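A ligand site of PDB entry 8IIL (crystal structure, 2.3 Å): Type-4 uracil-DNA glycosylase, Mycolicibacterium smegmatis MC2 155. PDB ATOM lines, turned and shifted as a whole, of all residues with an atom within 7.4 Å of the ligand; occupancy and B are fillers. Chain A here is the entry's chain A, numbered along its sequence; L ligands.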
ATOM      1  N   VAL A  36      23.675  21.905  26.381  1.00  0.00           N
ATOM      2  CA  VAL A  36      22.733  22.855  25.731  1.00  0.00           C
ATOM      3  C   VAL A  36      23.550  24.062  25.287  1.00  0.00           C
ATOM      4  O   VAL A  36      23.884  24.903  26.100  1.00  0.00           O
ATOM      5  CB  VAL A  36      21.508  23.179  26.599  1.00  0.00           C
ATOM      6  CG1 VAL A  36      20.541  24.120  25.896  1.00  0.00           C
ATOM      7  CG2 VAL A  36      20.796  21.920  27.041  1.00  0.00           C
ATOM      8  N   ILE A  49      22.751  36.079  27.354  1.00  0.00           N
ATOM      9  CA  ILE A  49      23.358  35.027  28.208  1.00  0.00           C
ATOM     10  C   ILE A  49      22.496  34.809  29.450  1.00  0.00           C
ATOM     11  O   ILE A  49      22.344  35.731  30.229  1.00  0.00           O
ATOM     12  CB  ILE A  49      24.824  35.328  28.550  1.00  0.00           C
ATOM     13  CG1 ILE A  49      25.671  35.708  27.334  1.00  0.00           C
ATOM     14  CG2 ILE A  49      25.437  34.186  29.345  1.00  0.00           C
ATOM     15  CD1 ILE A  49      27.046  36.190  27.687  1.00  0.00           C
ATOM     16  N   GLY A  50      21.903  33.635  29.550  1.00  0.00           N
ATOM     17  CA  GLY A  50      21.184  33.280  30.778  1.00  0.00           C
ATOM     18  C   GLY A  50      22.120  32.551  31.745  1.00  0.00           C
ATOM     19  O   GLY A  50      23.335  32.698  31.658  1.00  0.00           O
ATOM     20  N   GLU A  51      21.553  31.796  32.669  1.00  0.00           N
ATOM     21  CA  GLU A  51      22.360  31.131  33.729  1.00  0.00           C
ATOM     22  C   GLU A  51      22.689  29.710  33.298  1.00  0.00           C
ATOM     23  O   GLU A  51      23.879  29.390  33.246  1.00  0.00           O
ATOM     24  CB  GLU A  51      21.594  31.203  35.043  1.00  0.00           C
ATOM     25  CG  GLU A  51      21.988  30.194  36.103  1.00  0.00           C
ATOM     26  CD  GLU A  51      21.191  30.300  37.389  1.00  0.00           C
ATOM     27  OE1 GLU A  51      21.388  31.275  38.127  1.00  0.00           O
ATOM     28  OE2 GLU A  51      20.386  29.405  37.666  1.00  0.00           O
ATOM     29  N   GLN A  52      21.655  28.934  32.979  1.00  0.00           N
ATOM     30  CA  GLN A  52      21.827  27.494  32.661  1.00  0.00           C
ATOM     31  C   GLN A  52      20.571  26.968  31.977  1.00  0.00           C
ATOM     32  O   GLN A  52      19.499  27.522  32.185  1.00  0.00           O
ATOM     33  CB  GLN A  52      22.014  26.652  33.925  1.00  0.00           C
ATOM     34  CG  GLN A  52      20.890  26.704  34.939  1.00  0.00           C
ATOM     35  CD  GLN A  52      21.108  25.667  36.008  1.00  0.00           C
ATOM     36  OE1 GLN A  52      21.789  24.669  35.789  1.00  0.00           O
ATOM     37  NE2 GLN A  52      20.536  25.896  37.176  1.00  0.00           N
ATOM     38  N   PRO A  53      20.629  25.875  31.158  1.00  0.00           N
ATOM     39  CA  PRO A  53      19.410  25.268  30.671  1.00  0.00           C
ATOM     40  C   PRO A  53      18.554  24.754  31.848  1.00  0.00           C
ATOM     41  O   PRO A  53      19.111  24.393  32.836  1.00  0.00           O
ATOM     42  CB  PRO A  53      19.882  24.034  29.902  1.00  0.00           C
ATOM     43  CG  PRO A  53      21.266  23.762  30.399  1.00  0.00           C
ATOM     44  CD  PRO A  53      21.800  25.156  30.592  1.00  0.00           C
ATOM     45  N   GLY A  54      17.237  24.803  31.729  1.00  0.00           N
ATOM     46  CA  GLY A  54      16.344  24.202  32.737  1.00  0.00           C
ATOM     47  C   GLY A  54      15.926  22.795  32.326  1.00  0.00           C
ATOM     48  O   GLY A  54      16.612  22.185  31.522  1.00  0.00           O
ATOM     49  N   ASP A  55      14.802  22.311  32.834  1.00  0.00           N
ATOM     50  CA  ASP A  55      14.326  20.911  32.599  1.00  0.00           C
ATOM     51  C   ASP A  55      13.930  20.647  31.131  1.00  0.00           C
ATOM     52  O   ASP A  55      14.390  19.658  30.598  1.00  0.00           O
ATOM     53  CB  ASP A  55      13.398  20.527  33.766  1.00  0.00           C
ATOM     54  CG  ASP A  55      12.550  19.281  33.660  1.00  0.00           C
ATOM     55  OD1 ASP A  55      13.087  18.220  33.345  1.00  0.00           O
ATOM     56  OD2 ASP A  55      11.355  19.388  33.973  1.00  0.00           O
ATOM     57  N   GLU A  57      14.820  22.546  28.381  1.00  0.00           N
ATOM     58  CA  GLU A  57      16.044  22.817  27.564  1.00  0.00           C
ATOM     59  C   GLU A  57      16.957  21.586  27.581  1.00  0.00           C
ATOM     60  O   GLU A  57      17.442  21.236  26.515  1.00  0.00           O
ATOM     61  CB  GLU A  57      16.706  24.106  28.092  1.00  0.00           C
ATOM     62  CG  GLU A  57      15.918  25.371  27.924  1.00  0.00           C
ATOM     63  CD  GLU A  57      14.890  25.718  28.989  1.00  0.00           C
ATOM     64  OE1 GLU A  57      14.885  25.065  30.025  1.00  0.00           O
ATOM     65  OE2 GLU A  57      14.102  26.632  28.757  1.00  0.00           O
ATOM     66  N   LEU A  62      17.924  23.060  23.243  1.00  0.00           N
ATOM     67  CA  LEU A  62      17.886  24.495  22.865  1.00  0.00           C
ATOM     68  C   LEU A  62      17.684  25.360  24.100  1.00  0.00           C
ATOM     69  O   LEU A  62      16.925  24.958  24.961  1.00  0.00           O
ATOM     70  CB  LEU A  62      16.742  24.760  21.877  1.00  0.00           C
ATOM     71  CG  LEU A  62      16.881  24.138  20.490  1.00  0.00           C
ATOM     72  CD1 LEU A  62      15.524  24.002  19.827  1.00  0.00           C
ATOM     73  CD2 LEU A  62      17.834  24.937  19.624  1.00  0.00           C
ATOM     74  N   PRO A  63      18.297  26.560  24.172  1.00  0.00           N
ATOM     75  CA  PRO A  63      18.044  27.470  25.284  1.00  0.00           C
ATOM     76  C   PRO A  63      16.663  28.166  25.320  1.00  0.00           C
ATOM     77  O   PRO A  63      16.073  28.282  24.275  1.00  0.00           O
ATOM     78  CB  PRO A  63      19.160  28.509  25.089  1.00  0.00           C
ATOM     79  CG  PRO A  63      19.383  28.536  23.606  1.00  0.00           C
ATOM     80  CD  PRO A  63      19.245  27.080  23.196  1.00  0.00           C
ATOM     81  N   PHE A  64      16.152  28.510  26.503  1.00  0.00           N
ATOM     82  CA  PHE A  64      14.913  29.316  26.684  1.00  0.00           C
ATOM     83  C   PHE A  64      13.714  28.772  25.867  1.00  0.00           C
ATOM     84  O   PHE A  64      13.227  29.502  25.004  1.00  0.00           O
ATOM     85  CB  PHE A  64      15.264  30.797  26.486  1.00  0.00           C
ATOM     86  CG  PHE A  64      16.073  31.480  27.567  1.00  0.00           C
ATOM     87  CD1 PHE A  64      15.516  31.791  28.792  1.00  0.00           C
ATOM     88  CD2 PHE A  64      17.394  31.839  27.339  1.00  0.00           C
ATOM     89  CE1 PHE A  64      16.259  32.429  29.773  1.00  0.00           C
ATOM     90  CE2 PHE A  64      18.133  32.482  28.312  1.00  0.00           C
ATOM     91  CZ  PHE A  64      17.568  32.775  29.533  1.00  0.00           C
ATOM     92  N   VAL A  65      13.265  27.542  26.127  1.00  0.00           N
ATOM     93  CA  VAL A  65      12.120  26.901  25.406  1.00  0.00           C
ATOM     94  C   VAL A  65      10.982  26.676  26.411  1.00  0.00           C
ATOM     95  O   VAL A  65       9.912  26.255  25.982  1.00  0.00           O
ATOM     96  CB  VAL A  65      12.513  25.622  24.653  1.00  0.00           C
ATOM     97  CG1 VAL A  65      13.390  25.927  23.447  1.00  0.00           C
ATOM     98  CG2 VAL A  65      13.182  24.597  25.551  1.00  0.00           C
ATOM     99  N   GLY A  66      11.217  26.966  27.690  1.00  0.00           N
ATOM    100  CA  GLY A  66      10.180  26.830  28.728  1.00  0.00           C
ATOM    101  C   GLY A  66       9.495  28.132  29.109  1.00  0.00           C
ATOM    102  O   GLY A  66       9.488  29.063  28.313  1.00  0.00           O
ATOM    103  N   PRO A  67       8.866  28.225  30.298  1.00  0.00           N
ATOM    104  CA  PRO A  67       8.137  29.424  30.722  1.00  0.00           C
ATOM    105  C   PRO A  67       8.910  30.758  30.761  1.00  0.00           C
ATOM    106  O   PRO A  67       8.376  31.756  30.379  1.00  0.00           O
ATOM    107  CB  PRO A  67       7.558  29.017  32.101  1.00  0.00           C
ATOM    108  CG  PRO A  67       8.379  27.836  32.549  1.00  0.00           C
ATOM    109  CD  PRO A  67       8.784  27.132  31.274  1.00  0.00           C
ATOM    110  N   ALA A  68      10.173  30.739  31.186  1.00  0.00           N
ATOM    111  CA  ALA A  68      11.016  31.952  31.205  1.00  0.00           C
ATOM    112  C   ALA A  68      11.327  32.391  29.775  1.00  0.00           C
ATOM    113  O   ALA A  68      11.374  33.587  29.542  1.00  0.00           O
ATOM    114  CB  ALA A  68      12.256  31.698  32.009  1.00  0.00           C
ATOM    115  N   GLY A  69      11.508  31.444  28.861  1.00  0.00           N
ATOM    116  CA  GLY A  69      11.713  31.761  27.445  1.00  0.00           C
ATOM    117  C   GLY A  69      10.480  32.370  26.812  1.00  0.00           C
ATOM    118  O   GLY A  69      10.648  33.283  26.009  1.00  0.00           O
ATOM    119  N   VAL A  88      21.458  33.388  21.473  1.00  0.00           N
ATOM    120  CA  VAL A  88      20.959  33.170  22.858  1.00  0.00           C
ATOM    121  C   VAL A  88      21.677  31.960  23.486  1.00  0.00           C
ATOM    122  O   VAL A  88      21.574  30.906  22.919  1.00  0.00           O
ATOM    123  CB  VAL A  88      19.422  32.999  22.820  1.00  0.00           C
ATOM    124  CG1 VAL A  88      18.831  32.715  24.192  1.00  0.00           C
ATOM    125  CG2 VAL A  88      18.728  34.188  22.182  1.00  0.00           C
ATOM    126  N   THR A  89      22.320  32.122  24.642  1.00  0.00           N
ATOM    127  CA  THR A  89      23.079  31.059  25.334  1.00  0.00           C
ATOM    128  C   THR A  89      23.000  31.189  26.863  1.00  0.00           C
ATOM    129  O   THR A  89      22.225  32.013  27.319  1.00  0.00           O
ATOM    130  CB  THR A  89      24.530  30.968  24.814  1.00  0.00           C
ATOM    131  OG1 THR A  89      25.159  29.762  25.243  1.00  0.00           O
ATOM    132  CG2 THR A  89      25.366  32.184  25.151  1.00  0.00           C
ATOM    133  N   ASN A  90      23.801  30.406  27.589  1.00  0.00           N
ATOM    134  CA  ASN A  90      23.878  30.437  29.068  1.00  0.00           C
ATOM    135  C   ASN A  90      25.335  30.381  29.565  1.00  0.00           C
ATOM    136  O   ASN A  90      26.194  30.037  28.774  1.00  0.00           O
ATOM    137  CB  ASN A  90      23.026  29.326  29.696  1.00  0.00           C
ATOM    138  CG  ASN A  90      21.572  29.363  29.310  1.00  0.00           C
ATOM    139  OD1 ASN A  90      20.871  30.312  29.622  1.00  0.00           O
ATOM    140  ND2 ASN A  90      21.100  28.345  28.608  1.00  0.00           N
ATOM    141  N   ALA A  91      25.557  30.665  30.846  1.00  0.00           N
ATOM    142  CA  ALA A  91      26.894  30.693  31.478  1.00  0.00           C
ATOM    143  C   ALA A  91      27.407  29.267  31.648  1.00  0.00           C
ATOM    144  O   ALA A  91      28.577  29.062  31.407  1.00  0.00           O
ATOM    145  CB  ALA A  91      26.739  31.412  32.787  1.00  0.00           C
ATOM    146  N   VAL A  92      26.550  28.351  32.108  1.00  0.00           N
ATOM    147  CA  VAL A  92      26.883  26.910  32.197  1.00  0.00           C
ATOM    148  C   VAL A  92      25.999  26.186  31.156  1.00  0.00           C
ATOM    149  O   VAL A  92      24.890  26.665  30.922  1.00  0.00           O
ATOM    150  CB  VAL A  92      26.795  26.408  33.661  1.00  0.00           C
ATOM    151  CG1 VAL A  92      27.351  27.430  34.629  1.00  0.00           C
ATOM    152  CG2 VAL A  92      25.431  25.929  34.079  1.00  0.00           C
ATOM    153  N   LEU A 138      21.317  38.240  31.366  1.00  0.00           N
ATOM    154  CA  LEU A 138      20.027  37.940  32.018  1.00  0.00           C
ATOM    155  C   LEU A 138      20.246  37.327  33.404  1.00  0.00           C
ATOM    156  O   LEU A 138      20.489  36.130  33.475  1.00  0.00           O
ATOM    157  CB  LEU A 138      19.213  37.025  31.092  1.00  0.00           C
ATOM    158  CG  LEU A 138      18.842  37.597  29.721  1.00  0.00           C
ATOM    159  CD1 LEU A 138      18.617  36.471  28.729  1.00  0.00           C
ATOM    160  CD2 LEU A 138      17.605  38.469  29.813  1.00  0.00           C
ATOM    161  N   HIS A 177      16.686  38.388  35.479  1.00  0.00           N
ATOM    162  CA  HIS A 177      16.457  37.068  34.853  1.00  0.00           C
ATOM    163  C   HIS A 177      14.962  36.924  34.578  1.00  0.00           C
ATOM    164  O   HIS A 177      14.200  37.142  35.491  1.00  0.00           O
ATOM    165  CB  HIS A 177      16.983  35.954  35.751  1.00  0.00           C
ATOM    166  CG  HIS A 177      17.065  34.642  35.067  1.00  0.00           C
ATOM    167  ND1 HIS A 177      15.951  33.909  34.734  1.00  0.00           N
ATOM    168  CD2 HIS A 177      18.121  33.930  34.607  1.00  0.00           C
ATOM    169  CE1 HIS A 177      16.308  32.807  34.121  1.00  0.00           C
ATOM    170  NE2 HIS A 177      17.624  32.798  34.042  1.00  0.00           N
ATOM    171  N   PRO A 178      14.532  36.535  33.355  1.00  0.00           N
ATOM    172  CA  PRO A 178      13.109  36.415  32.985  1.00  0.00           C
ATOM    173  C   PRO A 178      12.255  35.534  33.933  1.00  0.00           C
ATOM    174  O   PRO A 178      11.086  35.782  34.000  1.00  0.00           O
ATOM    175  CB  PRO A 178      13.163  35.947  31.520  1.00  0.00           C
ATOM    176  CG  PRO A 178      14.519  35.316  31.370  1.00  0.00           C
ATOM    177  CD  PRO A 178      15.405  36.179  32.225  1.00  0.00           C
ATOM    178  N   SER A 179      12.854  34.587  34.661  1.00  0.00           N
ATOM    179  CA  SER A 179      12.131  33.734  35.646  1.00  0.00           C
ATOM    180  C   SER A 179      11.641  34.546  36.845  1.00  0.00           C
ATOM    181  O   SER A 179      10.734  34.094  37.520  1.00  0.00           O
ATOM    182  CB  SER A 179      12.986  32.574  36.076  1.00  0.00           C
ATOM    183  OG  SER A 179      13.992  32.996  36.985  1.00  0.00           O
HETATM  184  N1  LIG L   1      16.731  29.721  32.343  1.00  0.00           N
HETATM  185  C1  LIG L   1      17.957  30.097  31.879  1.00  0.00           C
HETATM  186  O1  LIG L   1      18.740  30.775  32.534  1.00  0.00           O
HETATM  187  N2  LIG L   1      18.272  29.660  30.632  1.00  0.00           N
HETATM  188  C2  LIG L   1      17.499  28.880  29.814  1.00  0.00           C
HETATM  189  O2  LIG L   1      17.920  28.561  28.709  1.00  0.00           O
HETATM  190  C3  LIG L   1      16.225  28.525  30.384  1.00  0.00           C
HETATM  191  C4  LIG L   1      15.892  28.952  31.609  1.00  0.00           C
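A ring nitrogen (ND1) of His 177 sits at hydrogen-bond distance from the side-chain hydroxyl (OG) of Ser 179 (3.1 Å). N of Glu 51 is in hydrogen-bond range of OD1 of Asn 90, at 3.5 Å. OD1 of Asn 90 sits close to N of Gly 50. O of Glu 51 is in hydrogen-bond range of N of Ala 91 (3.2 Å). The backbone NH of Val 92 lies within hydrogen-bond range of the backbone carbonyl oxygen of Glu 51, at 3.1 Å. The backbone NH of Gly 54 sits at hydrogen-bond distance from the side-chain carboxylate of Glu 57. The side-chain carboxylate (OE2) of Glu 57 lies within hydrogen-bond range of the backbone NH (N) of Gly 66 (3.1 Å). O of Thr 89 sits at hydrogen-bond distance from N of Gly 50, at 2.8 Å.
Gly 50 touches the ligand. Glu 57 touches the ligand (OE2 to C3, 3.3 Å). Pro 63 touches the ligand. Within 4 Å of the ligand: Gly 50, Glu 51, Gln 52, Glu 57, Pro 63, Phe 64, Asn 90 and His 177.
O1 of the ligand is in hydrogen-bond range of NE2 of His 177 (2.8 Å). The backbone NH (N) of Phe 64 lies within hydrogen-bond range of an oxygen (O2) of the ligand. OD1 of Asn 90 sits at hydrogen-bond distance from N2 of the ligand (2.9 Å). The backbone NH (N) of Gln 52 is in hydrogen-bond range of an oxygen (O1) of the ligand (3.5 Å). O of Gln 52 lies within hydrogen-bond range of N2 of the ligand. The backbone NH (N) of Glu 51 lies within hydrogen-bond range of an oxygen (O1) of the ligand (3.0 Å).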
